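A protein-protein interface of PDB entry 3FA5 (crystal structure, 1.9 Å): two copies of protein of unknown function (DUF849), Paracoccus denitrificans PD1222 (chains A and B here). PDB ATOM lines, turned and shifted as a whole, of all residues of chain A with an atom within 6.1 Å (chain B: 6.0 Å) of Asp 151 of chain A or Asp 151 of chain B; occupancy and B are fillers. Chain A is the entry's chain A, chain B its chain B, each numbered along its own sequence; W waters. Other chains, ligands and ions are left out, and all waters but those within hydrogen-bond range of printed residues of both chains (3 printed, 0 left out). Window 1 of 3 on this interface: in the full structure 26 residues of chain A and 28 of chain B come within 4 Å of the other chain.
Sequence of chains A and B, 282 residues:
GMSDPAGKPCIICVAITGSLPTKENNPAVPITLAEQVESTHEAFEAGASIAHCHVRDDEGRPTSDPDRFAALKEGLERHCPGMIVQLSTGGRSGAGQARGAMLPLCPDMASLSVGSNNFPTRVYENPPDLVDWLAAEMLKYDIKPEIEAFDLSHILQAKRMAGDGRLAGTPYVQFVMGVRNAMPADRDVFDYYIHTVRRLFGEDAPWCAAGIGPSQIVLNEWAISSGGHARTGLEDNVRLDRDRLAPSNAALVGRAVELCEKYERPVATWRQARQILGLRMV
A ring nitrogen (NE2) of His 154 of chain A lies within hydrogen-bond range of the backbone carbonyl oxygen (O) of Ser 116 of chain A, at 3.0 Å.
NE2 of His 154 of chain B is in hydrogen-bond range of O of Ser 116 of chain B (3.0 Å).
N of Phe 150 of chain B sits at hydrogen-bond distance from ND1 of His 154 of chain B, 3.4 Å away.
Among the printed residues, pairs that only touch across the chains: Ser 116 of chain A with Ser 116 of chain B, Ser 116 of chain A with Asn 117 of chain B, Asn 117 of chain A with Ser 116 of chain B, Asp 151 of chain A with His 154 of chain B, Leu 152 of chain A with Leu 152 of chain B, Leu 152 of chain A with Met 183 of chain B, Ser 153 of chain A with Ala 182 of chain B, Ser 153 of chain A with Met 183 of chain B, Ala 182 of chain A with Ser 153 of chain B, Met 183 of chain A with Leu 152 of chain B and Met 183 of chain A with Ser 153 of chain B.
The side-chain carboxylate (OD1) of Asp 151 of chain A lies within hydrogen-bond range of the backbone NH (N) of Leu 152 of chain B (3.4 Å).
The side-chain hydroxyl (OG) of Ser 153 of chain B is in hydrogen-bond range of the side-chain carboxylate (OD2) of Asp 151 of chain A, at 2.4 Å.
N of Leu 152 of chain A lies within hydrogen-bond range of OD1 of Asp 151 of chain B, at 3.5 Å.
The side-chain hydroxyl of Ser 153 of chain A lies within hydrogen-bond range of the side-chain carboxylate of Asp 151 of chain B.
The side-chain carboxylate (OD1) of Asp 151 of chain A lies close to the side-chain carboxylate (OD1) of Asp 151 of chain B (3.2 Å).
Hydrophobic or aromatic side chains of chain B within 4 Å of the printed part of chain A: Leu 152, His 154 and Met 183.
Ser 116 of chain A touches its own counterpart, Ser 116 of chain B.
Asp 151 of chain A touches its own counterpart, Asp 151 of chain B.
Asp 151 of chain A touches His 154 of chain B, but with the chains exchanged His 154 of chain A does not touch Asp 151 of chain B (4.04 Å).
Leu 152 of chain A touches Met 183 of chain B, and with the chains exchanged Met 183 of chain A touches Leu 152 of chain B.
Positions printed for both chains: 116, 117, 148, 149, 150, 151, 152, 153, 154, 155, 176, 182, 183 and 193.
Of the 16 pairs that touch across the chains among the printed residues, 15 have their exchanged pair printed and touching as well.
Water W3 lies within hydrogen-bond range of OD2 of Asp 151 of chain B (2.5 Å), O of Ser 116 of chain A (3.0 Å) and NE2 of His 154 of chain A (3.2 Å).
Water W2 lies within hydrogen-bond range of OD2 of Asp 151 of chain A (2.6 Å), O of Ser 116 of chain B (3.2 Å), NE2 of His 154 of chain B (3.2 Å) and OG of Ser 153 of chain B (3.5 Å).
Water W1 lies within hydrogen-bond range of O of Phe 150 of chain B (2.9 Å), OG of Ser 153 of chain A (3.1 Å) and OD2 of Asp 151 of chain B (3.3 Å).
Of chain B, only Asp 151, Leu 152, Ser 153 and His 154 come within 4 Å of Asp 151 of chain A.
Asp 151 of chain B touches just these residues of chain A: Asp 151, Leu 152 and Ser 153.
Printed residues of chain B within 4 Å of Ser 153 of chain A: Asp 151 (2.6 Å), Ala 182 (3.5 Å) and Met 183 (3.5 Å).
Of the printed residues of chain A, Ser 116 of chain B touches Ser 116 and Asn 117.
Printed residues of chain A within 4 Å of Ala 182 of chain B: Ser 153 (3.5 Å).
Of the printed residues of chain B, Leu 152 of chain A touches Asp 151, Leu 152 and Met 183.
Of the printed residues of chain A, Ser 153 of chain B touches Asp 151 (2.4 Å), Ala 182 (3.5 Å) and Met 183 (3.6 Å).
The nearest residue of chain B that does not touch Asp 151 of chain A is Ser 116 of chain B (5.4 Å).
The nearest residue of chain A that does not touch Asp 151 of chain B is His 154 of chain A (4.04 Å).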
ATOM      1  N   SER A 116      -1.144  -2.925  -1.475  1.00  0.00           N
ATOM      2  CA  SER A 116      -1.040  -4.129  -2.261  1.00  0.00           C
ATOM      3  C   SER A 116      -0.801  -3.750  -3.728  1.00  0.00           C
ATOM      4  O   SER A 116      -0.931  -2.588  -4.113  1.00  0.00           O
ATOM      5  CB  SER A 116      -2.251  -5.040  -2.046  1.00  0.00           C
ATOM      6  OG  SER A 116      -2.413  -5.407  -0.648  1.00  0.00           O
ATOM      7  N   ASN A 117      -0.354  -4.727  -4.505  1.00  0.00           N
ATOM      8  CA  ASN A 117      -0.016  -4.535  -5.891  1.00  0.00           C
ATOM      9  C   ASN A 117       0.221  -5.901  -6.483  1.00  0.00           C
ATOM     10  O   ASN A 117       0.251  -6.913  -5.769  1.00  0.00           O
ATOM     11  CB  ASN A 117       1.255  -3.701  -6.031  1.00  0.00           C
ATOM     12  CG  ASN A 117       2.419  -4.276  -5.227  1.00  0.00           C
ATOM     13  OD1 ASN A 117       2.541  -4.023  -4.028  1.00  0.00           O
ATOM     14  ND2 ASN A 117       3.257  -5.075  -5.880  1.00  0.00           N
ATOM     15  N   GLU A 148       8.264  -0.065   1.723  1.00  0.00           N
ATOM     16  CA  GLU A 148       8.614  -0.560   0.398  1.00  0.00           C
ATOM     17  C   GLU A 148       7.429  -0.208  -0.506  1.00  0.00           C
ATOM     18  O   GLU A 148       6.407  -0.876  -0.499  1.00  0.00           O
ATOM     19  CB  GLU A 148       8.872  -2.066   0.442  1.00  0.00           C
ATOM     20  CG  GLU A 148       9.978  -2.437   1.397  1.00  0.00           C
ATOM     21  CD  GLU A 148      10.447  -3.876   1.256  1.00  0.00           C
ATOM     22  OE1 GLU A 148       9.586  -4.780   1.136  1.00  0.00           O
ATOM     23  OE2 GLU A 148      11.687  -4.099   1.283  1.00  0.00           O
ATOM     24  N   ALA A 149       7.584   0.916  -1.202  1.00  0.00           N
ATOM     25  CA  ALA A 149       6.564   1.505  -2.040  1.00  0.00           C
ATOM     26  C   ALA A 149       6.640   0.969  -3.461  1.00  0.00           C
ATOM     27  O   ALA A 149       7.533   1.354  -4.230  1.00  0.00           O
ATOM     28  CB  ALA A 149       6.700   3.071  -2.026  1.00  0.00           C
ATOM     29  N   PHE A 150       5.698   0.085  -3.793  1.00  0.00           N
ATOM     30  CA  PHE A 150       5.547  -0.495  -5.128  1.00  0.00           C
ATOM     31  C   PHE A 150       4.662   0.315  -6.081  1.00  0.00           C
ATOM     32  O   PHE A 150       4.592  -0.023  -7.292  1.00  0.00           O
ATOM     33  CB  PHE A 150       4.955  -1.922  -5.069  1.00  0.00           C
ATOM     34  CG  PHE A 150       5.895  -2.917  -4.480  1.00  0.00           C
ATOM     35  CD1 PHE A 150       6.815  -3.566  -5.275  1.00  0.00           C
ATOM     36  CD2 PHE A 150       5.890  -3.161  -3.109  1.00  0.00           C
ATOM     37  CE1 PHE A 150       7.715  -4.469  -4.728  1.00  0.00           C
ATOM     38  CE2 PHE A 150       6.780  -4.059  -2.545  1.00  0.00           C
ATOM     39  CZ  PHE A 150       7.698  -4.716  -3.356  1.00  0.00           C
ATOM     40  N   ASP A 151       3.944   1.309  -5.545  1.00  0.00           N
ATOM     41  CA  ASP A 151       3.098   2.167  -6.369  1.00  0.00           C
ATOM     42  C   ASP A 151       2.899   3.529  -5.711  1.00  0.00           C
ATOM     43  O   ASP A 151       3.149   3.669  -4.500  1.00  0.00           O
ATOM     44  CB  ASP A 151       1.723   1.499  -6.638  1.00  0.00           C
ATOM     45  CG  ASP A 151       1.200   1.816  -8.034  1.00  0.00           C
ATOM     46  OD1 ASP A 151       1.616   2.861  -8.595  1.00  0.00           O
ATOM     47  OD2 ASP A 151       0.447   0.989  -8.591  1.00  0.00           O
ATOM     48  N   LEU A 152       2.453   4.507  -6.498  1.00  0.00           N
ATOM     49  CA  LEU A 152       2.248   5.874  -6.005  1.00  0.00           C
ATOM     50  C   LEU A 152       1.384   5.998  -4.741  1.00  0.00           C
ATOM     51  O   LEU A 152       1.770   6.703  -3.810  1.00  0.00           O
ATOM     52  CB  LEU A 152       1.682   6.789  -7.075  1.00  0.00           C
ATOM     53  CG  LEU A 152       1.525   8.265  -6.692  1.00  0.00           C
ATOM     54  CD1 LEU A 152       2.900   8.896  -6.247  1.00  0.00           C
ATOM     55  CD2 LEU A 152       0.878   9.047  -7.800  1.00  0.00           C
ATOM     56  N   SER A 153       0.201   5.379  -4.710  1.00  0.00           N
ATOM     57  CA  SER A 153      -0.647   5.493  -3.513  1.00  0.00           C
ATOM     58  C   SER A 153      -0.028   4.929  -2.237  1.00  0.00           C
ATOM     59  O   SER A 153      -0.488   5.209  -1.145  1.00  0.00           O
ATOM     60  CB  SER A 153      -2.009   4.831  -3.729  1.00  0.00           C
ATOM     61  OG  SER A 153      -1.967   3.426  -3.543  1.00  0.00           O
ATOM     62  N   HIS A 154       0.939   4.056  -2.350  1.00  0.00           N
ATOM     63  CA  HIS A 154       1.575   3.506  -1.153  1.00  0.00           C
ATOM     64  C   HIS A 154       2.235   4.687  -0.371  1.00  0.00           C
ATOM     65  O   HIS A 154       2.209   4.714   0.895  1.00  0.00           O
ATOM     66  CB  HIS A 154       2.589   2.422  -1.556  1.00  0.00           C
ATOM     67  CG  HIS A 154       1.964   1.241  -2.225  1.00  0.00           C
ATOM     68  ND1 HIS A 154       2.653   0.083  -2.488  1.00  0.00           N
ATOM     69  CD2 HIS A 154       0.689   1.013  -2.632  1.00  0.00           C
ATOM     70  CE1 HIS A 154       1.850  -0.790  -3.069  1.00  0.00           C
ATOM     71  NE2 HIS A 154       0.644  -0.256  -3.155  1.00  0.00           N
ATOM     72  N   ILE A 155       2.775   5.664  -1.135  1.00  0.00           N
ATOM     73  CA  ILE A 155       3.505   6.813  -0.554  1.00  0.00           C
ATOM     74  C   ILE A 155       2.498   7.715   0.150  1.00  0.00           C
ATOM     75  O   ILE A 155       2.664   8.044   1.356  1.00  0.00           O
ATOM     76  CB  ILE A 155       4.345   7.595  -1.611  1.00  0.00           C
ATOM     77  CG1 ILE A 155       5.255   6.629  -2.406  1.00  0.00           C
ATOM     78  CG2 ILE A 155       5.190   8.719  -0.920  1.00  0.00           C
ATOM     79  CD1 ILE A 155       6.098   7.351  -3.556  1.00  0.00           C
ATOM     80  N   VAL A 176      10.369   1.073  -5.146  1.00  0.00           N
ATOM     81  CA  VAL A 176      10.700  -0.221  -5.788  1.00  0.00           C
ATOM     82  C   VAL A 176      10.216  -0.225  -7.263  1.00  0.00           C
ATOM     83  O   VAL A 176       9.030  -0.085  -7.539  1.00  0.00           O
ATOM     84  CB  VAL A 176      10.119  -1.411  -4.982  1.00  0.00           C
ATOM     85  CG1 VAL A 176      10.801  -2.701  -5.341  1.00  0.00           C
ATOM     86  CG2 VAL A 176      10.257  -1.127  -3.484  1.00  0.00           C
ATOM     87  N   ALA A 182       4.038  -4.564 -11.782  1.00  0.00           N
ATOM     88  CA  ALA A 182       3.933  -3.419 -10.842  1.00  0.00           C
ATOM     89  C   ALA A 182       4.477  -2.153 -11.522  1.00  0.00           C
ATOM     90  O   ALA A 182       3.997  -1.782 -12.577  1.00  0.00           O
ATOM     91  CB  ALA A 182       4.692  -3.724  -9.596  1.00  0.00           C
ATOM     92  N   MET A 183       5.494  -1.504 -10.949  1.00  0.00           N
ATOM     93  CA  MET A 183       5.941  -0.226 -11.481  1.00  0.00           C
ATOM     94  C   MET A 183       7.188  -0.422 -12.301  1.00  0.00           C
ATOM     95  O   MET A 183       8.224  -0.872 -11.809  1.00  0.00           O
ATOM     96  CB  MET A 183       6.182   0.786 -10.369  1.00  0.00           C
ATOM     97  CG  MET A 183       6.588   2.098 -10.881  1.00  0.00           C
ATOM     98  SD  MET A 183       5.238   2.989 -11.885  1.00  0.00           S
ATOM     99  CE  MET A 183       4.105   3.564 -10.351  1.00  0.00           C
ATOM    100  N   TYR A 193       8.007  10.593  -7.810  1.00  0.00           N
ATOM    101  CA  TYR A 193       8.144  10.000  -6.497  1.00  0.00           C
ATOM    102  C   TYR A 193       8.986  10.918  -5.558  1.00  0.00           C
ATOM    103  O   TYR A 193       8.645  11.108  -4.402  1.00  0.00           O
ATOM    104  CB  TYR A 193       8.803   8.634  -6.617  1.00  0.00           C
ATOM    105  CG  TYR A 193       7.926   7.465  -6.980  1.00  0.00           C
ATOM    106  CD1 TYR A 193       6.534   7.560  -7.103  1.00  0.00           C
ATOM    107  CD2 TYR A 193       8.504   6.229  -7.114  1.00  0.00           C
ATOM    108  CE1 TYR A 193       5.756   6.388  -7.368  1.00  0.00           C
ATOM    109  CE2 TYR A 193       7.791   5.100  -7.389  1.00  0.00           C
ATOM    110  CZ  TYR A 193       6.404   5.160  -7.508  1.00  0.00           C
ATOM    111  OH  TYR A 193       5.751   3.980  -7.788  1.00  0.00           O
ATOM    112  N   SER B 116      -3.607  -4.720  -8.942  1.00  0.00           N
ATOM    113  CA  SER B 116      -4.295  -4.882  -7.672  1.00  0.00           C
ATOM    114  C   SER B 116      -3.988  -3.657  -6.760  1.00  0.00           C
ATOM    115  O   SER B 116      -3.180  -2.762  -7.101  1.00  0.00           O
ATOM    116  CB  SER B 116      -3.959  -6.240  -7.022  1.00  0.00           C
ATOM    117  OG  SER B 116      -4.304  -7.359  -7.863  1.00  0.00           O
ATOM    118  N   ASN B 117      -4.729  -3.564  -5.663  1.00  0.00           N
ATOM    119  CA  ASN B 117      -4.630  -2.407  -4.753  1.00  0.00           C
ATOM    120  C   ASN B 117      -5.445  -2.716  -3.515  1.00  0.00           C
ATOM    121  O   ASN B 117      -6.296  -3.603  -3.535  1.00  0.00           O
ATOM    122  CB  ASN B 117      -5.142  -1.100  -5.393  1.00  0.00           C
ATOM    123  CG  ASN B 117      -6.556  -1.236  -5.946  1.00  0.00           C
ATOM    124  OD1 ASN B 117      -6.737  -1.651  -7.088  1.00  0.00           O
ATOM    125  ND2 ASN B 117      -7.548  -0.928  -5.126  1.00  0.00           N
ATOM    126  N   GLU B 148     -10.082   0.704 -15.202  1.00  0.00           N
ATOM    127  CA  GLU B 148     -10.286   1.345 -13.914  1.00  0.00           C
ATOM    128  C   GLU B 148      -8.933   1.387 -13.144  1.00  0.00           C
ATOM    129  O   GLU B 148      -8.576   0.445 -12.433  1.00  0.00           O
ATOM    130  CB  GLU B 148     -11.434   0.661 -13.144  1.00  0.00           C
ATOM    131  CG  GLU B 148     -12.786   0.637 -13.970  1.00  0.00           C
ATOM    132  CD  GLU B 148     -13.995  -0.031 -13.244  1.00  0.00           C
ATOM    133  OE1 GLU B 148     -13.807  -0.862 -12.327  1.00  0.00           O
ATOM    134  OE2 GLU B 148     -15.154   0.288 -13.608  1.00  0.00           O
ATOM    135  N   ALA B 149      -8.182   2.482 -13.373  1.00  0.00           N
ATOM    136  CA  ALA B 149      -6.864   2.746 -12.757  1.00  0.00           C
ATOM    137  C   ALA B 149      -7.008   3.238 -11.317  1.00  0.00           C
ATOM    138  O   ALA B 149      -7.486   4.361 -11.069  1.00  0.00           O
ATOM    139  CB  ALA B 149      -6.088   3.759 -13.611  1.00  0.00           C
ATOM    140  N   PHE B 150      -6.684   2.363 -10.366  1.00  0.00           N
ATOM    141  CA  PHE B 150      -6.697   2.655  -8.923  1.00  0.00           C
ATOM    142  C   PHE B 150      -5.364   3.178  -8.361  1.00  0.00           C
ATOM    143  O   PHE B 150      -5.277   3.618  -7.196  1.00  0.00           O
ATOM    144  CB  PHE B 150      -7.083   1.409  -8.126  1.00  0.00           C
ATOM    145  CG  PHE B 150      -8.542   1.166  -8.108  1.00  0.00           C
ATOM    146  CD1 PHE B 150      -9.347   1.846  -7.196  1.00  0.00           C
ATOM    147  CD2 PHE B 150      -9.123   0.364  -9.064  1.00  0.00           C
ATOM    148  CE1 PHE B 150     -10.714   1.661  -7.200  1.00  0.00           C
ATOM    149  CE2 PHE B 150     -10.479   0.192  -9.077  1.00  0.00           C
ATOM    150  CZ  PHE B 150     -11.276   0.837  -8.136  1.00  0.00           C
ATOM    151  N   ASP B 151      -4.333   3.079  -9.173  1.00  0.00           N
ATOM    152  CA  ASP B 151      -2.991   3.539  -8.806  1.00  0.00           C
ATOM    153  C   ASP B 151      -2.201   3.866 -10.060  1.00  0.00           C
ATOM    154  O   ASP B 151      -2.639   3.535 -11.173  1.00  0.00           O
ATOM    155  CB  ASP B 151      -2.290   2.478  -7.985  1.00  0.00           C
ATOM    156  CG  ASP B 151      -1.469   3.066  -6.914  1.00  0.00           C
ATOM    157  OD1 ASP B 151      -0.957   4.180  -7.155  1.00  0.00           O
ATOM    158  OD2 ASP B 151      -1.336   2.427  -5.829  1.00  0.00           O
ATOM    159  N   LEU B 152      -1.083   4.553  -9.916  1.00  0.00           N
ATOM    160  CA  LEU B 152      -0.380   5.067 -11.096  1.00  0.00           C
ATOM    161  C   LEU B 152       0.137   3.919 -11.950  1.00  0.00           C
ATOM    162  O   LEU B 152       0.027   3.995 -13.167  1.00  0.00           O
ATOM    163  CB  LEU B 152       0.784   6.041 -10.729  1.00  0.00           C
ATOM    164  CG  LEU B 152       1.846   6.494 -11.723  1.00  0.00           C
ATOM    165  CD1 LEU B 152       1.288   7.447 -12.845  1.00  0.00           C
ATOM    166  CD2 LEU B 152       3.039   7.141 -10.930  1.00  0.00           C
ATOM    167  N   SER B 153       0.711   2.877 -11.328  1.00  0.00           N
ATOM    168  CA  SER B 153       1.350   1.771 -12.103  1.00  0.00           C
ATOM    169  C   SER B 153       0.346   1.118 -13.067  1.00  0.00           C
ATOM    170  O   SER B 153       0.727   0.679 -14.159  1.00  0.00           O
ATOM    171  CB  SER B 153       1.967   0.725 -11.185  1.00  0.00           C
ATOM    172  OG  SER B 153       0.996  -0.156 -10.661  1.00  0.00           O
ATOM    173  N   HIS B 154      -0.940   1.153 -12.684  1.00  0.00           N
ATOM    174  CA  HIS B 154      -2.035   0.568 -13.454  1.00  0.00           C
ATOM    175  C   HIS B 154      -2.105   1.223 -14.808  1.00  0.00           C
ATOM    176  O   HIS B 154      -2.266   0.518 -15.797  1.00  0.00           O
ATOM    177  CB  HIS B 154      -3.386   0.708 -12.736  1.00  0.00           C
ATOM    178  CG  HIS B 154      -3.444  -0.003 -11.412  1.00  0.00           C
ATOM    179  ND1 HIS B 154      -4.630  -0.268 -10.767  1.00  0.00           N
ATOM    180  CD2 HIS B 154      -2.469  -0.507 -10.622  1.00  0.00           C
ATOM    181  CE1 HIS B 154      -4.385  -0.897  -9.626  1.00  0.00           C
ATOM    182  NE2 HIS B 154      -3.078  -1.064  -9.513  1.00  0.00           N
ATOM    183  N   ILE B 155      -1.945   2.546 -14.835  1.00  0.00           N
ATOM    184  CA  ILE B 155      -1.833   3.311 -16.088  1.00  0.00           C
ATOM    185  C   ILE B 155      -0.631   2.871 -16.934  1.00  0.00           C
ATOM    186  O   ILE B 155      -0.773   2.660 -18.147  1.00  0.00           O
ATOM    187  CB  ILE B 155      -1.765   4.847 -15.870  1.00  0.00           C
ATOM    188  CG1 ILE B 155      -2.885   5.319 -14.978  1.00  0.00           C
ATOM    189  CG2 ILE B 155      -1.840   5.631 -17.220  1.00  0.00           C
ATOM    190  CD1 ILE B 155      -2.906   6.826 -14.759  1.00  0.00           C
ATOM    191  N   VAL B 176      -9.491   6.419 -10.756  1.00  0.00           N
ATOM    192  CA  VAL B 176     -10.439   6.211  -9.665  1.00  0.00           C
ATOM    193  C   VAL B 176      -9.868   6.723  -8.362  1.00  0.00           C
ATOM    194  O   VAL B 176      -8.876   6.184  -7.856  1.00  0.00           O
ATOM    195  CB  VAL B 176     -10.806   4.755  -9.436  1.00  0.00           C
ATOM    196  CG1 VAL B 176     -11.900   4.691  -8.338  1.00  0.00           C
ATOM    197  CG2 VAL B 176     -11.282   4.065 -10.757  1.00  0.00           C
ATOM    198  N   ALA B 182      -6.502   3.237  -0.918  1.00  0.00           N
ATOM    199  CA  ALA B 182      -6.062   3.239  -2.307  1.00  0.00           C
ATOM    200  C   ALA B 182      -5.586   4.680  -2.573  1.00  0.00           C
ATOM    201  O   ALA B 182      -4.825   5.207  -1.771  1.00  0.00           O
ATOM    202  CB  ALA B 182      -7.205   2.833  -3.216  1.00  0.00           C
ATOM    203  N   MET B 183      -6.067   5.330  -3.632  1.00  0.00           N
ATOM    204  CA  MET B 183      -5.672   6.688  -3.948  1.00  0.00           C
ATOM    205  C   MET B 183      -6.726   7.666  -3.483  1.00  0.00           C
ATOM    206  O   MET B 183      -7.848   7.653  -3.984  1.00  0.00           O
ATOM    207  CB  MET B 183      -5.496   6.865  -5.470  1.00  0.00           C
ATOM    208  CG  MET B 183      -4.918   8.198  -5.843  1.00  0.00           C
ATOM    209  SD  MET B 183      -3.148   8.405  -5.317  1.00  0.00           S
ATOM    210  CE  MET B 183      -2.262   7.193  -6.503  1.00  0.00           C
ATOM    211  N   TYR B 193      -1.595  12.154 -13.283  1.00  0.00           N
ATOM    212  CA  TYR B 193      -2.340  11.166 -14.067  1.00  0.00           C
ATOM    213  C   TYR B 193      -2.639  11.687 -15.499  1.00  0.00           C
ATOM    214  O   TYR B 193      -2.444  10.990 -16.490  1.00  0.00           O
ATOM    215  CB  TYR B 193      -3.647  10.877 -13.348  1.00  0.00           C
ATOM    216  CG  TYR B 193      -3.595   9.886 -12.210  1.00  0.00           C
ATOM    217  CD1 TYR B 193      -2.447   9.171 -11.900  1.00  0.00           C
ATOM    218  CD2 TYR B 193      -4.767   9.544 -11.560  1.00  0.00           C
ATOM    219  CE1 TYR B 193      -2.495   8.170 -10.903  1.00  0.00           C
ATOM    220  CE2 TYR B 193      -4.807   8.573 -10.548  1.00  0.00           C
ATOM    221  CZ  TYR B 193      -3.683   7.903 -10.234  1.00  0.00           C
ATOM    222  OH  TYR B 193      -3.797   6.907  -9.296  1.00  0.00           O
HETATM  223  O   HOH W   1      -4.478   2.101  -4.867  1.00  0.00           O
HETATM  224  O   HOH W   2      -0.425  -1.304  -7.692  1.00  0.00           O
HETATM  225  O   HOH W   3      -1.967   0.167  -4.898  1.00  0.00           O
